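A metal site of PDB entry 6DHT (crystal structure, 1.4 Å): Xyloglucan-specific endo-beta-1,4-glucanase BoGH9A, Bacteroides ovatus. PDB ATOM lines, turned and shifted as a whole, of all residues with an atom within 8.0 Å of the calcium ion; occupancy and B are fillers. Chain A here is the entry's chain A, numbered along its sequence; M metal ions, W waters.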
ATOM      1  N   PHE A 197      34.322   6.377  16.285  1.00  0.00           N
ATOM      2  CA  PHE A 197      33.283   6.371  15.282  1.00  0.00           C
ATOM      3  C   PHE A 197      32.214   5.304  15.513  1.00  0.00           C
ATOM      4  O   PHE A 197      31.073   5.476  15.088  1.00  0.00           O
ATOM      5  CB  PHE A 197      33.897   6.297  13.899  1.00  0.00           C
ATOM      6  CG  PHE A 197      34.582   7.566  13.510  1.00  0.00           C
ATOM      7  CD1 PHE A 197      33.858   8.727  13.274  1.00  0.00           C
ATOM      8  CD2 PHE A 197      35.951   7.625  13.394  1.00  0.00           C
ATOM      9  CE1 PHE A 197      34.495   9.916  12.943  1.00  0.00           C
ATOM     10  CE2 PHE A 197      36.597   8.816  13.060  1.00  0.00           C
ATOM     11  CZ  PHE A 197      35.860   9.945  12.832  1.00  0.00           C
ATOM     12  N   SER A 198      32.563   4.233  16.216  1.00  0.00           N
ATOM     13  CA  SER A 198      31.572   3.218  16.534  1.00  0.00           C
ATOM     14  C   SER A 198      30.535   3.754  17.503  1.00  0.00           C
ATOM     15  O   SER A 198      29.353   3.455  17.382  1.00  0.00           O
ATOM     16  CB  SER A 198      32.251   1.981  17.129  1.00  0.00           C
ATOM     17  OG  SER A 198      31.272   1.005  17.444  1.00  0.00           O
ATOM     18  N   GLN A 200      29.848   7.088  17.948  1.00  0.00           N
ATOM     19  CA  GLN A 200      29.241   8.332  17.462  1.00  0.00           C
ATOM     20  C   GLN A 200      27.859   8.078  16.892  1.00  0.00           C
ATOM     21  O   GLN A 200      27.717   7.235  16.036  1.00  0.00           O
ATOM     22  CB  GLN A 200      30.146   8.915  16.395  1.00  0.00           C
ATOM     23  CG  GLN A 200      29.699  10.261  15.810  1.00  0.00           C
ATOM     24  CD  GLN A 200      30.527  10.660  14.613  1.00  0.00           C
ATOM     25  OE1 GLN A 200      30.852   9.855  13.748  1.00  0.00           O
ATOM     26  NE2 GLN A 200      30.837  11.958  14.541  1.00  0.00           N
ATOM     27  N   LYS A 201      26.870   8.834  17.324  1.00  0.00           N
ATOM     28  CA  LYS A 201      25.541   8.742  16.721  1.00  0.00           C
ATOM     29  C   LYS A 201      25.034  10.133  16.377  1.00  0.00           C
ATOM     30  O   LYS A 201      24.984  11.026  17.210  1.00  0.00           O
ATOM     31  CB  LYS A 201      24.560   7.989  17.641  1.00  0.00           C
ATOM     32  CG  LYS A 201      24.931   6.495  17.858  1.00  0.00           C
ATOM     33  CD  LYS A 201      24.834   5.673  16.553  1.00  0.00           C
ATOM     34  CE  LYS A 201      25.235   4.214  16.754  1.00  0.00           C
ATOM     35  NZ  LYS A 201      26.518   4.042  17.500  1.00  0.00           N
ATOM     36  N   ILE A 202      24.685  10.308  15.109  1.00  0.00           N
ATOM     37  CA  ILE A 202      24.371  11.645  14.584  1.00  0.00           C
ATOM     38  C   ILE A 202      22.929  11.811  14.106  1.00  0.00           C
ATOM     39  O   ILE A 202      22.590  12.816  13.454  1.00  0.00           O
ATOM     40  CB  ILE A 202      25.330  12.047  13.447  1.00  0.00           C
ATOM     41  CG1 ILE A 202      25.281  11.048  12.293  1.00  0.00           C
ATOM     42  CG2 ILE A 202      26.759  12.149  13.976  1.00  0.00           C
ATOM     43  CD1 ILE A 202      25.973  11.521  11.036  1.00  0.00           C
ATOM     44  N   ILE A 204      20.914  10.067  11.897  1.00  0.00           N
ATOM     45  CA  ILE A 204      20.602   9.858  10.494  1.00  0.00           C
ATOM     46  C   ILE A 204      19.722   8.605  10.405  1.00  0.00           C
ATOM     47  O   ILE A 204      19.597   7.864  11.380  1.00  0.00           O
ATOM     48  CB  ILE A 204      21.875   9.700   9.633  1.00  0.00           C
ATOM     49  CG1 ILE A 204      22.815   8.636  10.204  1.00  0.00           C
ATOM     50  CG2 ILE A 204      22.589  11.036   9.527  1.00  0.00           C
ATOM     51  CD1 ILE A 204      23.968   8.275   9.292  1.00  0.00           C
ATOM     52  N   PRO A 205      19.107   8.350   9.243  1.00  0.00           N
ATOM     53  CA  PRO A 205      18.219   7.189   9.151  1.00  0.00           C
ATOM     54  C   PRO A 205      18.908   5.870   9.527  1.00  0.00           C
ATOM     55  O   PRO A 205      18.248   4.937   9.990  1.00  0.00           O
ATOM     56  CB  PRO A 205      17.773   7.208   7.689  1.00  0.00           C
ATOM     57  CG  PRO A 205      17.843   8.654   7.317  1.00  0.00           C
ATOM     58  CD  PRO A 205      19.062   9.170   8.030  1.00  0.00           C
ATOM     59  N   GLU A 206      20.227   5.835   9.373  1.00  0.00           N
ATOM     60  CA  GLU A 206      21.009   4.622   9.590  1.00  0.00           C
ATOM     61  C   GLU A 206      21.599   4.559  11.008  1.00  0.00           C
ATOM     62  O   GLU A 206      22.463   3.701  11.283  1.00  0.00           O
ATOM     63  CB  GLU A 206      22.105   4.477   8.524  1.00  0.00           C
ATOM     64  CG  GLU A 206      21.584   4.561   7.071  1.00  0.00           C
ATOM     65  CD  GLU A 206      21.292   5.975   6.559  1.00  0.00           C
ATOM     66  OE1 GLU A 206      21.622   6.973   7.245  1.00  0.00           O
ATOM     67  OE2 GLU A 206      20.719   6.088   5.445  1.00  0.00           O
ATOM     68  N   SER A 207      21.160   5.434  11.896  1.00  0.00           N
ATOM     69  CA  SER A 207      21.731   5.494  13.244  1.00  0.00           C
ATOM     70  C   SER A 207      21.393   4.294  14.129  1.00  0.00           C
ATOM     71  O   SER A 207      22.051   4.093  15.134  1.00  0.00           O
ATOM     72  CB  SER A 207      21.358   6.781  13.978  1.00  0.00           C
ATOM     73  OG  SER A 207      22.047   7.905  13.433  1.00  0.00           O
ATOM     74  N   ASN A 208      20.404   3.500  13.736  1.00  0.00           N
ATOM     75  CA  ASN A 208      20.030   2.348  14.582  1.00  0.00           C
ATOM     76  C   ASN A 208      20.392   1.002  13.988  1.00  0.00           C
ATOM     77  O   ASN A 208      19.950  -0.041  14.481  1.00  0.00           O
ATOM     78  CB  ASN A 208      18.543   2.415  14.941  1.00  0.00           C
ATOM     79  CG  ASN A 208      18.228   3.588  15.859  1.00  0.00           C
ATOM     80  OD1 ASN A 208      17.281   4.336  15.620  1.00  0.00           O
ATOM     81  ND2 ASN A 208      19.038   3.770  16.895  1.00  0.00           N
ATOM     82  N   ASN A 209      21.249   0.988  12.966  1.00  0.00           N
ATOM     83  CA  ASN A 209      21.729  -0.264  12.417  1.00  0.00           C
ATOM     84  C   ASN A 209      23.017  -0.699  13.121  1.00  0.00           C
ATOM     85  O   ASN A 209      23.346  -0.166  14.165  1.00  0.00           O
ATOM     86  CB  ASN A 209      21.892  -0.185  10.899  1.00  0.00           C
ATOM     87  CG  ASN A 209      23.046   0.699  10.452  1.00  0.00           C
ATOM     88  OD1 ASN A 209      23.892   1.122  11.247  1.00  0.00           O
ATOM     89  ND2 ASN A 209      23.071   0.971   9.161  1.00  0.00           N
ATOM     90  N   HIS A 210      23.745  -1.637  12.533  1.00  0.00           N
ATOM     91  CA  HIS A 210      24.943  -2.205  13.158  1.00  0.00           C
ATOM     92  C   HIS A 210      26.255  -1.669  12.597  1.00  0.00           C
ATOM     93  O   HIS A 210      27.323  -2.246  12.816  1.00  0.00           O
ATOM     94  CB  HIS A 210      24.924  -3.740  13.041  1.00  0.00           C
ATOM     95  CG  HIS A 210      23.913  -4.392  13.935  1.00  0.00           C
ATOM     96  ND1 HIS A 210      22.553  -4.249  13.749  1.00  0.00           N
ATOM     97  CD2 HIS A 210      24.066  -5.181  15.016  1.00  0.00           C
ATOM     98  CE1 HIS A 210      21.908  -4.926  14.678  1.00  0.00           C
ATOM     99  NE2 HIS A 210      22.799  -5.502  15.464  1.00  0.00           N
ATOM    100  N   THR A 211      26.171  -0.547  11.878  1.00  0.00           N
ATOM    101  CA  THR A 211      27.322  -0.014  11.147  1.00  0.00           C
ATOM    102  C   THR A 211      27.626   1.384  11.689  1.00  0.00           C
ATOM    103  O   THR A 211      26.700   2.137  11.971  1.00  0.00           O
ATOM    104  CB  THR A 211      27.008   0.063   9.660  1.00  0.00           C
ATOM    105  OG1 THR A 211      26.653  -1.262   9.194  1.00  0.00           O
ATOM    106  CG2 THR A 211      28.235   0.509   8.884  1.00  0.00           C
ATOM    107  N   PRO A 212      28.912   1.703  11.869  1.00  0.00           N
ATOM    108  CA  PRO A 212      29.234   3.096  12.254  1.00  0.00           C
ATOM    109  C   PRO A 212      28.642   4.112  11.282  1.00  0.00           C
ATOM    110  O   PRO A 212      28.712   3.955  10.055  1.00  0.00           O
ATOM    111  CB  PRO A 212      30.775   3.124  12.203  1.00  0.00           C
ATOM    112  CG  PRO A 212      31.173   1.678  12.517  1.00  0.00           C
ATOM    113  CD  PRO A 212      30.126   0.871  11.761  1.00  0.00           C
ATOM    114  N   ASP A 213      28.048   5.131  11.864  1.00  0.00           N
ATOM    115  CA  ASP A 213      27.300   6.132  11.106  1.00  0.00           C
ATOM    116  C   ASP A 213      28.165   6.845  10.058  1.00  0.00           C
ATOM    117  O   ASP A 213      27.657   7.148   8.986  1.00  0.00           O
ATOM    118  CB  ASP A 213      26.648   7.165  12.032  1.00  0.00           C
ATOM    119  CG  ASP A 213      25.401   6.659  12.725  1.00  0.00           C
ATOM    120  OD1 ASP A 213      25.041   5.473  12.551  1.00  0.00           O
ATOM    121  OD2 ASP A 213      24.792   7.451  13.465  1.00  0.00           O
ATOM    122  N   LEU A 214      29.449   7.096  10.338  1.00  0.00           N
ATOM    123  CA  LEU A 214      30.324   7.653   9.323  1.00  0.00           C
ATOM    124  C   LEU A 214      30.341   6.765   8.086  1.00  0.00           C
ATOM    125  O   LEU A 214      30.254   7.269   6.968  1.00  0.00           O
ATOM    126  CB  LEU A 214      31.746   7.897   9.820  1.00  0.00           C
ATOM    127  CG  LEU A 214      32.712   8.504   8.812  1.00  0.00           C
ATOM    128  CD1 LEU A 214      33.712   9.387   9.573  1.00  0.00           C
ATOM    129  CD2 LEU A 214      33.425   7.497   7.974  1.00  0.00           C
ATOM    130  N   LEU A 215      30.419   5.437   8.276  1.00  0.00           N
ATOM    131  CA  LEU A 215      30.439   4.541   7.130  1.00  0.00           C
ATOM    132  C   LEU A 215      29.083   4.482   6.441  1.00  0.00           C
ATOM    133  O   LEU A 215      29.040   4.409   5.220  1.00  0.00           O
ATOM    134  CB  LEU A 215      30.840   3.131   7.558  1.00  0.00           C
ATOM    135  CG  LEU A 215      32.282   2.965   8.036  1.00  0.00           C
ATOM    136  CD1 LEU A 215      32.586   1.473   8.306  1.00  0.00           C
ATOM    137  CD2 LEU A 215      33.310   3.559   7.068  1.00  0.00           C
ATOM    138  N   ASP A 216      27.984   4.534   7.188  1.00  0.00           N
ATOM    139  CA  ASP A 216      26.669   4.661   6.535  1.00  0.00           C
ATOM    140  C   ASP A 216      26.638   5.847   5.585  1.00  0.00           C
ATOM    141  O   ASP A 216      26.148   5.759   4.439  1.00  0.00           O
ATOM    142  CB  ASP A 216      25.533   4.806   7.524  1.00  0.00           C
ATOM    143  CG  ASP A 216      25.311   3.565   8.381  1.00  0.00           C
ATOM    144  OD1 ASP A 216      25.198   2.441   7.826  1.00  0.00           O
ATOM    145  OD2 ASP A 216      25.231   3.756   9.599  1.00  0.00           O
ATOM    146  N   GLU A 217      27.125   6.978   6.069  1.00  0.00           N
ATOM    147  CA  GLU A 217      27.099   8.173   5.252  1.00  0.00           C
ATOM    148  C   GLU A 217      27.965   8.018   4.004  1.00  0.00           C
ATOM    149  O   GLU A 217      27.517   8.332   2.894  1.00  0.00           O
ATOM    150  CB  GLU A 217      27.520   9.408   6.047  1.00  0.00           C
ATOM    151  CG  GLU A 217      27.205  10.724   5.307  1.00  0.00           C
ATOM    152  CD  GLU A 217      25.712  10.884   5.036  1.00  0.00           C
ATOM    153  OE1 GLU A 217      24.920  10.785   5.998  1.00  0.00           O
ATOM    154  OE2 GLU A 217      25.327  11.063   3.848  1.00  0.00           O
ATOM    155  N   ASP A 288      24.598  -5.177   7.135  1.00  0.00           N
ATOM    156  CA  ASP A 288      23.912  -4.002   6.634  1.00  0.00           C
ATOM    157  C   ASP A 288      24.260  -3.696   5.179  1.00  0.00           C
ATOM    158  O   ASP A 288      23.487  -3.075   4.467  1.00  0.00           O
ATOM    159  CB  ASP A 288      24.275  -2.803   7.515  1.00  0.00           C
ATOM    160  CG  ASP A 288      23.637  -2.880   8.896  1.00  0.00           C
ATOM    161  OD1 ASP A 288      22.532  -3.465   9.059  1.00  0.00           O
ATOM    162  OD2 ASP A 288      24.231  -2.351   9.863  1.00  0.00           O
ATOM    163  N   TYR A 289      25.436  -4.126   4.752  1.00  0.00           N
ATOM    164  CA  TYR A 289      25.880  -3.890   3.371  1.00  0.00           C
ATOM    165  C   TYR A 289      26.334  -5.178   2.678  1.00  0.00           C
ATOM    166  O   TYR A 289      27.489  -5.334   2.311  1.00  0.00           O
ATOM    167  CB  TYR A 289      26.956  -2.788   3.352  1.00  0.00           C
ATOM    168  CG  TYR A 289      26.391  -1.490   3.872  1.00  0.00           C
ATOM    169  CD1 TYR A 289      25.644  -0.659   3.054  1.00  0.00           C
ATOM    170  CD2 TYR A 289      26.557  -1.130   5.200  1.00  0.00           C
ATOM    171  CE1 TYR A 289      25.082   0.491   3.532  1.00  0.00           C
ATOM    172  CE2 TYR A 289      25.994   0.050   5.690  1.00  0.00           C
ATOM    173  CZ  TYR A 289      25.253   0.852   4.843  1.00  0.00           C
ATOM    174  OH  TYR A 289      24.674   2.018   5.287  1.00  0.00           O
HETATM  175 CA    CA M   1      24.718   3.267  11.785  1.00  0.00          CA
HETATM  176  O   HOH W   1      24.328   2.635  14.023  1.00  0.00           O
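The backbone carbonyl oxygen (O) of Thr 211 binds the calcium ion, 2.3 Å away. OD2 of Asp 216 binds the calcium ion (2.3 Å). The calcium ion is bound by O of Glu 206, 2.4 Å away. The calcium ion is bound by the side-chain carboxylate (OD1) of Asp 213. The calcium ion is bound by water W1 (2.4 Å). The calcium ion is bound by OD1 of Asn 209 (2.4 Å). The calcium ion has six donor atoms within binding distance.
OD2 of Asp 213 lies within hydrogen-bond range of N of Ile 202 (3.3 Å). The side-chain hydroxyl (OG1) of Thr 211 is in hydrogen-bond range of the side-chain carboxylate (OD2) of Asp 288. The side-chain carboxylate (OD2) of Asp 213 sits at hydrogen-bond distance from the side-chain hydroxyl (OG) of Ser 207 (2.8 Å). The side-chain carboxylate (OD1) of Asp 216 lies within hydrogen-bond range of the side-chain hydroxyl (OH) of Tyr 289 (2.6 Å).
Of the 21 residues printed, 5 come within 4 Å of the calcium ion. The nearest printed residue that does not touch the calcium ion is Ser 207 (4.001 Å).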
